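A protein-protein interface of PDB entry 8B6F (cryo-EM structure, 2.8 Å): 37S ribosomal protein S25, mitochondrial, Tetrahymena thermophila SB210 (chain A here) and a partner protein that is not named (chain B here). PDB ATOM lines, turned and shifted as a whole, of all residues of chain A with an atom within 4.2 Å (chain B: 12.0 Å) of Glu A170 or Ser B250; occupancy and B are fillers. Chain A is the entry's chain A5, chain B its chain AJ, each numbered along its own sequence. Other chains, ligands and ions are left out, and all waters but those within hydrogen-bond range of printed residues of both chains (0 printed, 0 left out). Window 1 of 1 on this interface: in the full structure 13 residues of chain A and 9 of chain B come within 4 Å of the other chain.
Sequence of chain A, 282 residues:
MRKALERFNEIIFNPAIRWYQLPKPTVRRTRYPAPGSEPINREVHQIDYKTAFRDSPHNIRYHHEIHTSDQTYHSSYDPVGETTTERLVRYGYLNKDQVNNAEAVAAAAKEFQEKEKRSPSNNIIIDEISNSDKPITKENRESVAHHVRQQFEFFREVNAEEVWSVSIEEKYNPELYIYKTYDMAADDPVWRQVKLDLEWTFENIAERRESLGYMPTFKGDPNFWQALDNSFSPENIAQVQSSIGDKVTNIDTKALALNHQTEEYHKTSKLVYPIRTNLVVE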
ATOM      1  N   SER A 167     -24.669 -15.302 -18.000  1.00  0.00           N
ATOM      2  CA  SER A 167     -24.203 -15.472 -16.626  1.00  0.00           C
ATOM      3  C   SER A 167     -25.217 -16.332 -15.885  1.00  0.00           C
ATOM      4  O   SER A 167     -26.343 -15.888 -15.646  1.00  0.00           O
ATOM      5  CB  SER A 167     -24.021 -14.121 -15.947  1.00  0.00           C
ATOM      6  OG  SER A 167     -23.595 -14.277 -14.605  1.00  0.00           O
ATOM      7  N   ILE A 168     -24.816 -17.552 -15.522  1.00  0.00           N
ATOM      8  CA  ILE A 168     -25.697 -18.432 -14.762  1.00  0.00           C
ATOM      9  C   ILE A 168     -25.982 -17.843 -13.389  1.00  0.00           C
ATOM     10  O   ILE A 168     -27.080 -18.012 -12.846  1.00  0.00           O
ATOM     11  CB  ILE A 168     -25.091 -19.846 -14.663  1.00  0.00           C
ATOM     12  CG1 ILE A 168     -26.126 -20.844 -14.137  1.00  0.00           C
ATOM     13  CG2 ILE A 168     -23.860 -19.851 -13.767  1.00  0.00           C
ATOM     14  CD1 ILE A 168     -27.275 -21.108 -15.090  1.00  0.00           C
ATOM     15  N   GLU A 169     -25.004 -17.152 -12.802  1.00  0.00           N
ATOM     16  CA  GLU A 169     -25.239 -16.468 -11.536  1.00  0.00           C
ATOM     17  C   GLU A 169     -26.337 -15.425 -11.676  1.00  0.00           C
ATOM     18  O   GLU A 169     -27.208 -15.307 -10.806  1.00  0.00           O
ATOM     19  CB  GLU A 169     -23.947 -15.819 -11.044  1.00  0.00           C
ATOM     20  CG  GLU A 169     -22.932 -16.802 -10.488  1.00  0.00           C
ATOM     21  CD  GLU A 169     -23.381 -17.424  -9.182  1.00  0.00           C
ATOM     22  OE1 GLU A 169     -24.455 -17.037  -8.676  1.00  0.00           O
ATOM     23  OE2 GLU A 169     -22.658 -18.298  -8.658  1.00  0.00           O
ATOM     24  N   GLU A 170     -26.318 -14.658 -12.767  1.00  0.00           N
ATOM     25  CA  GLU A 170     -27.392 -13.703 -13.011  1.00  0.00           C
ATOM     26  C   GLU A 170     -28.720 -14.419 -13.210  1.00  0.00           C
ATOM     27  O   GLU A 170     -29.764 -13.948 -12.743  1.00  0.00           O
ATOM     28  CB  GLU A 170     -27.059 -12.842 -14.229  1.00  0.00           C
ATOM     29  CG  GLU A 170     -28.162 -11.871 -14.642  1.00  0.00           C
ATOM     30  CD  GLU A 170     -28.519 -10.883 -13.548  1.00  0.00           C
ATOM     31  OE1 GLU A 170     -27.758 -10.780 -12.563  1.00  0.00           O
ATOM     32  OE2 GLU A 170     -29.562 -10.204 -13.674  1.00  0.00           O
ATOM     33  N   LYS A 171     -28.706 -15.556 -13.908  1.00  0.00           N
ATOM     34  CA  LYS A 171     -29.945 -16.293 -14.129  1.00  0.00           C
ATOM     35  C   LYS A 171     -30.568 -16.738 -12.811  1.00  0.00           C
ATOM     36  O   LYS A 171     -31.790 -16.667 -12.639  1.00  0.00           O
ATOM     37  CB  LYS A 171     -29.680 -17.502 -15.027  1.00  0.00           C
ATOM     38  CG  LYS A 171     -29.396 -17.152 -16.481  1.00  0.00           C
ATOM     39  CD  LYS A 171     -30.646 -16.660 -17.191  1.00  0.00           C
ATOM     40  CE  LYS A 171     -30.367 -16.369 -18.655  1.00  0.00           C
ATOM     41  NZ  LYS A 171     -31.594 -15.930 -19.376  1.00  0.00           N
ATOM     42  N   TYR A 172     -29.748 -17.210 -11.873  1.00  0.00           N
ATOM     43  CA  TYR A 172     -30.251 -17.774 -10.627  1.00  0.00           C
ATOM     44  C   TYR A 172     -30.363 -16.760  -9.497  1.00  0.00           C
ATOM     45  O   TYR A 172     -30.966 -17.077  -8.467  1.00  0.00           O
ATOM     46  CB  TYR A 172     -29.360 -18.936 -10.181  1.00  0.00           C
ATOM     47  CG  TYR A 172     -29.793 -20.260 -10.759  1.00  0.00           C
ATOM     48  CD1 TYR A 172     -29.334 -20.684 -11.998  1.00  0.00           C
ATOM     49  CD2 TYR A 172     -30.673 -21.080 -10.071  1.00  0.00           C
ATOM     50  CE1 TYR A 172     -29.738 -21.892 -12.531  1.00  0.00           C
ATOM     51  CE2 TYR A 172     -31.083 -22.288 -10.595  1.00  0.00           C
ATOM     52  CZ  TYR A 172     -30.611 -22.689 -11.825  1.00  0.00           C
ATOM     53  OH  TYR A 172     -31.016 -23.893 -12.351  1.00  0.00           O
ATOM     54  N   ASN A 173     -29.807 -15.561  -9.651  1.00  0.00           N
ATOM     55  CA  ASN A 173     -29.934 -14.495  -8.656  1.00  0.00           C
ATOM     56  C   ASN A 173     -30.264 -13.192  -9.371  1.00  0.00           C
ATOM     57  O   ASN A 173     -29.425 -12.290  -9.468  1.00  0.00           O
ATOM     58  CB  ASN A 173     -28.655 -14.356  -7.830  1.00  0.00           C
ATOM     59  CG  ASN A 173     -28.303 -15.626  -7.085  1.00  0.00           C
ATOM     60  OD1 ASN A 173     -29.182 -16.382  -6.675  1.00  0.00           O
ATOM     61  ND2 ASN A 173     -27.010 -15.865  -6.900  1.00  0.00           N
ATOM     62  N   PRO A 174     -31.484 -13.063  -9.888  1.00  0.00           N
ATOM     63  CA  PRO A 174     -31.829 -11.859 -10.652  1.00  0.00           C
ATOM     64  C   PRO A 174     -31.700 -10.601  -9.806  1.00  0.00           C
ATOM     65  O   PRO A 174     -32.014 -10.595  -8.614  1.00  0.00           O
ATOM     66  CB  PRO A 174     -33.282 -12.107 -11.076  1.00  0.00           C
ATOM     67  CG  PRO A 174     -33.486 -13.576 -10.941  1.00  0.00           C
ATOM     68  CD  PRO A 174     -32.608 -14.010  -9.814  1.00  0.00           C
ATOM     69  N   GLU A 175     -31.236  -9.529 -10.440  1.00  0.00           N
ATOM     70  CA  GLU A 175     -31.159  -8.210  -9.825  1.00  0.00           C
ATOM     71  C   GLU A 175     -32.045  -7.271 -10.629  1.00  0.00           C
ATOM     72  O   GLU A 175     -31.834  -7.098 -11.833  1.00  0.00           O
ATOM     73  CB  GLU A 175     -29.717  -7.701  -9.786  1.00  0.00           C
ATOM     74  CG  GLU A 175     -29.548  -6.336  -9.133  1.00  0.00           C
ATOM     75  CD  GLU A 175     -29.896  -6.338  -7.655  1.00  0.00           C
ATOM     76  OE1 GLU A 175     -30.110  -7.432  -7.090  1.00  0.00           O
ATOM     77  OE2 GLU A 175     -29.954  -5.244  -7.057  1.00  0.00           O
ATOM     78  N   TYR A 177     -34.341  -3.535 -11.130  1.00  0.00           N
ATOM     79  CA  TYR A 177     -34.532  -2.126 -10.829  1.00  0.00           C
ATOM     80  C   TYR A 177     -36.028  -1.868 -10.716  1.00  0.00           C
ATOM     81  O   TYR A 177     -36.785  -2.172 -11.643  1.00  0.00           O
ATOM     82  CB  TYR A 177     -33.913  -1.241 -11.909  1.00  0.00           C
ATOM     83  CG  TYR A 177     -34.178   0.228 -11.691  1.00  0.00           C
ATOM     84  CD1 TYR A 177     -33.364   0.984 -10.861  1.00  0.00           C
ATOM     85  CD2 TYR A 177     -35.247   0.856 -12.310  1.00  0.00           C
ATOM     86  CE1 TYR A 177     -33.608   2.324 -10.656  1.00  0.00           C
ATOM     87  CE2 TYR A 177     -35.498   2.193 -12.111  1.00  0.00           C
ATOM     88  CZ  TYR A 177     -34.676   2.922 -11.284  1.00  0.00           C
ATOM     89  OH  TYR A 177     -34.928   4.258 -11.089  1.00  0.00           O
ATOM     90  N   PRO B 246     -44.078  -1.268 -12.297  1.00  0.00           N
ATOM     91  CA  PRO B 246     -42.949  -1.226 -13.235  1.00  0.00           C
ATOM     92  C   PRO B 246     -41.679  -1.799 -12.623  1.00  0.00           C
ATOM     93  O   PRO B 246     -41.436  -1.693 -11.421  1.00  0.00           O
ATOM     94  CB  PRO B 246     -42.798   0.268 -13.548  1.00  0.00           C
ATOM     95  CG  PRO B 246     -43.473   0.969 -12.432  1.00  0.00           C
ATOM     96  CD  PRO B 246     -44.584   0.081 -11.990  1.00  0.00           C
ATOM     97  N   SER B 247     -40.865  -2.416 -13.476  1.00  0.00           N
ATOM     98  CA  SER B 247     -39.615  -3.021 -13.040  1.00  0.00           C
ATOM     99  C   SER B 247     -38.811  -3.437 -14.263  1.00  0.00           C
ATOM    100  O   SER B 247     -39.379  -3.750 -15.314  1.00  0.00           O
ATOM    101  CB  SER B 247     -39.868  -4.233 -12.137  1.00  0.00           C
ATOM    102  OG  SER B 247     -38.655  -4.876 -11.792  1.00  0.00           O
ATOM    103  N   LEU B 248     -37.488  -3.439 -14.113  1.00  0.00           N
ATOM    104  CA  LEU B 248     -36.581  -3.880 -15.162  1.00  0.00           C
ATOM    105  C   LEU B 248     -35.518  -4.783 -14.556  1.00  0.00           C
ATOM    106  O   LEU B 248     -35.251  -4.745 -13.354  1.00  0.00           O
ATOM    107  CB  LEU B 248     -35.914  -2.701 -15.883  1.00  0.00           C
ATOM    108  CG  LEU B 248     -36.786  -1.883 -16.838  1.00  0.00           C
ATOM    109  CD1 LEU B 248     -35.987  -0.736 -17.410  1.00  0.00           C
ATOM    110  CD2 LEU B 248     -37.343  -2.742 -17.959  1.00  0.00           C
ATOM    111  N   ARG B 249     -34.910  -5.599 -15.411  1.00  0.00           N
ATOM    112  CA  ARG B 249     -33.891  -6.563 -15.003  1.00  0.00           C
ATOM    113  C   ARG B 249     -32.522  -5.979 -15.341  1.00  0.00           C
ATOM    114  O   ARG B 249     -32.100  -5.993 -16.499  1.00  0.00           O
ATOM    115  CB  ARG B 249     -34.119  -7.899 -15.700  1.00  0.00           C
ATOM    116  CG  ARG B 249     -33.315  -9.052 -15.135  1.00  0.00           C
ATOM    117  CD  ARG B 249     -33.396 -10.258 -16.059  1.00  0.00           C
ATOM    118  NE  ARG B 249     -32.804 -11.454 -15.472  1.00  0.00           N
ATOM    119  CZ  ARG B 249     -33.475 -12.378 -14.797  1.00  0.00           C
ATOM    120  NH1 ARG B 249     -34.775 -12.273 -14.583  1.00  0.00           N
ATOM    121  NH2 ARG B 249     -32.823 -13.437 -14.325  1.00  0.00           N
ATOM    122  N   SER B 250     -31.828  -5.468 -14.327  1.00  0.00           N
ATOM    123  CA  SER B 250     -30.516  -4.872 -14.544  1.00  0.00           C
ATOM    124  C   SER B 250     -29.468  -5.951 -14.779  1.00  0.00           C
ATOM    125  O   SER B 250     -29.460  -6.988 -14.110  1.00  0.00           O
ATOM    126  CB  SER B 250     -30.113  -4.014 -13.346  1.00  0.00           C
ATOM    127  OG  SER B 250     -31.086  -3.022 -13.079  1.00  0.00           O
ATOM    128  N   ILE B 251     -28.570  -5.694 -15.725  1.00  0.00           N
ATOM    129  CA  ILE B 251     -27.506  -6.623 -16.085  1.00  0.00           C
ATOM    130  C   ILE B 251     -26.176  -5.895 -15.959  1.00  0.00           C
ATOM    131  O   ILE B 251     -26.025  -4.777 -16.465  1.00  0.00           O
ATOM    132  CB  ILE B 251     -27.688  -7.177 -17.510  1.00  0.00           C
ATOM    133  CG1 ILE B 251     -29.127  -7.654 -17.731  1.00  0.00           C
ATOM    134  CG2 ILE B 251     -26.706  -8.310 -17.762  1.00  0.00           C
ATOM    135  CD1 ILE B 251     -29.548  -8.816 -16.853  1.00  0.00           C
ATOM    136  N   LYS B 252     -25.219  -6.524 -15.283  1.00  0.00           N
ATOM    137  CA  LYS B 252     -23.870  -5.999 -15.139  1.00  0.00           C
ATOM    138  C   LYS B 252     -22.871  -7.111 -15.428  1.00  0.00           C
ATOM    139  O   LYS B 252     -23.233  -8.280 -15.579  1.00  0.00           O
ATOM    140  CB  LYS B 252     -23.636  -5.422 -13.737  1.00  0.00           C
ATOM    141  CG  LYS B 252     -23.898  -6.404 -12.606  1.00  0.00           C
ATOM    142  CD  LYS B 252     -23.422  -5.858 -11.266  1.00  0.00           C
ATOM    143  CE  LYS B 252     -24.140  -4.573 -10.892  1.00  0.00           C
ATOM    144  NZ  LYS B 252     -23.750  -4.105  -9.533  1.00  0.00           N
ATOM    145  N   LYS B 253     -21.598  -6.735 -15.505  1.00  0.00           N
ATOM    146  CA  LYS B 253     -20.549  -7.709 -15.758  1.00  0.00           C
ATOM    147  C   LYS B 253     -20.375  -8.641 -14.563  1.00  0.00           C
ATOM    148  O   LYS B 253     -20.723  -8.313 -13.424  1.00  0.00           O
ATOM    149  CB  LYS B 253     -19.227  -7.006 -16.065  1.00  0.00           C
ATOM    150  CG  LYS B 253     -19.238  -6.224 -17.365  1.00  0.00           C
ATOM    151  CD  LYS B 253     -17.881  -5.604 -17.643  1.00  0.00           C
ATOM    152  CE  LYS B 253     -17.839  -4.955 -19.013  1.00  0.00           C
ATOM    153  NZ  LYS B 253     -18.059  -5.944 -20.105  1.00  0.00           N
ATOM    154  N   LYS B 254     -19.826  -9.821 -14.836  1.00  0.00           N
ATOM    155  CA  LYS B 254     -19.600 -10.802 -13.785  1.00  0.00           C
ATOM    156  C   LYS B 254     -18.616 -10.264 -12.756  1.00  0.00           C
ATOM    157  O   LYS B 254     -17.677  -9.537 -13.089  1.00  0.00           O
ATOM    158  CB  LYS B 254     -19.067 -12.103 -14.383  1.00  0.00           C
ATOM    159  CG  LYS B 254     -19.994 -12.758 -15.391  1.00  0.00           C
ATOM    160  CD  LYS B 254     -19.322 -13.949 -16.056  1.00  0.00           C
ATOM    161  CE  LYS B 254     -20.237 -14.598 -17.080  1.00  0.00           C
ATOM    162  NZ  LYS B 254     -19.594 -15.769 -17.740  1.00  0.00           N
ATOM    163  N   TYR B 255     -18.837 -10.625 -11.496  1.00  0.00           N
ATOM    164  CA  TYR B 255     -17.940 -10.234 -10.416  1.00  0.00           C
ATOM    165  C   TYR B 255     -17.589 -11.441  -9.553  1.00  0.00           C
ATOM    166  O   TYR B 255     -18.278 -12.460  -9.578  1.00  0.00           O
ATOM    167  CB  TYR B 255     -18.573  -9.134  -9.561  1.00  0.00           C
ATOM    168  CG  TYR B 255     -19.898  -9.521  -8.949  1.00  0.00           C
ATOM    169  CD1 TYR B 255     -19.959 -10.150  -7.713  1.00  0.00           C
ATOM    170  CD2 TYR B 255     -21.090  -9.253  -9.608  1.00  0.00           C
ATOM    171  CE1 TYR B 255     -21.170 -10.505  -7.151  1.00  0.00           C
ATOM    172  CE2 TYR B 255     -22.306  -9.604  -9.056  1.00  0.00           C
ATOM    173  CZ  TYR B 255     -22.341 -10.229  -7.826  1.00  0.00           C
ATOM    174  OH  TYR B 255     -23.548 -10.580  -7.271  1.00  0.00           O
ATOM    175  OXT TYR B 255     -16.607 -11.430  -8.813  1.00  0.00           O
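Hydrophobic or aromatic side chains of chain B that line the printed part of chain A: Ile B251.
Of the 10 printed residues of chain A, 6 touch a printed residue of chain B.
Printed residues of chain A that touch a printed residue of chain B: Ser A167, Glu A170, Lys A171, Pro A174, Glu A175 and Tyr A177.
Hydrophobic or aromatic side chains of chain A within 4 Å of the printed part of chain B: Pro A174 and Tyr A177.
Among the printed residues, 11 pairs touch across the chains.
Among the printed residues, merely in contact across the chains: Pro A174 with Arg B249 (3.5 Å), Glu A170 with Ile B251 (3.5 Å), Tyr A177 with Ser B250 (3.5 Å), Glu A175 with Arg B249 (3.7 Å), Lys A171 with Arg B249 (3.8 Å) and Ser A167 with Lys B254 (3.98 Å).
OG of Ser A167 is in hydrogen-bond range of N of Glu A170, 3.3 Å away.
The side-chain carboxylate (OE2) of Glu A170 lies within salt-bridge range of the guanidinium group (NE) of Arg B249.
The side-chain carboxylate (OE2) of Glu A170 lies close to the backbone carbonyl oxygen (O) of Ser B250 (3.2 Å).
O of Leu B248 sits at hydrogen-bond distance from N of Tyr A177.
N of Ser B250 lies within hydrogen-bond range of O of Glu A175 (3.0 Å).
OG of Ser B247 sits close to O of Tyr A177.
No residue of chain B comes within 4 Å of Ile A168.
No residue of chain B comes within 4 Å of Glu A169.
Glu A170 touches three residues of chain B.
Lys A171 touches just one residue of chain B: Arg B249.
No residue of chain B comes within 4 Å of Asn A173.
Of the printed residues of chain B, Pro A174 touches Arg B249.
Glu A175 touches two residues of chain B.
Of the printed residues of chain B, Tyr A177 touches Ser B247 (3.3 Å), Leu B248 (2.7 Å) and Ser B250 (3.5 Å).
Printed residues of chain A within 4 Å of Leu B248: Tyr A177 (2.7 Å).
Of chain A, only Glu A170 (3.2 Å), Glu A175 (3.0 Å) and Tyr A177 (3.5 Å) come within 4 Å of Ser B250.
The nearest printed residue of chain A that does not touch Ser B250 is Pro A174 (6.0 Å).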
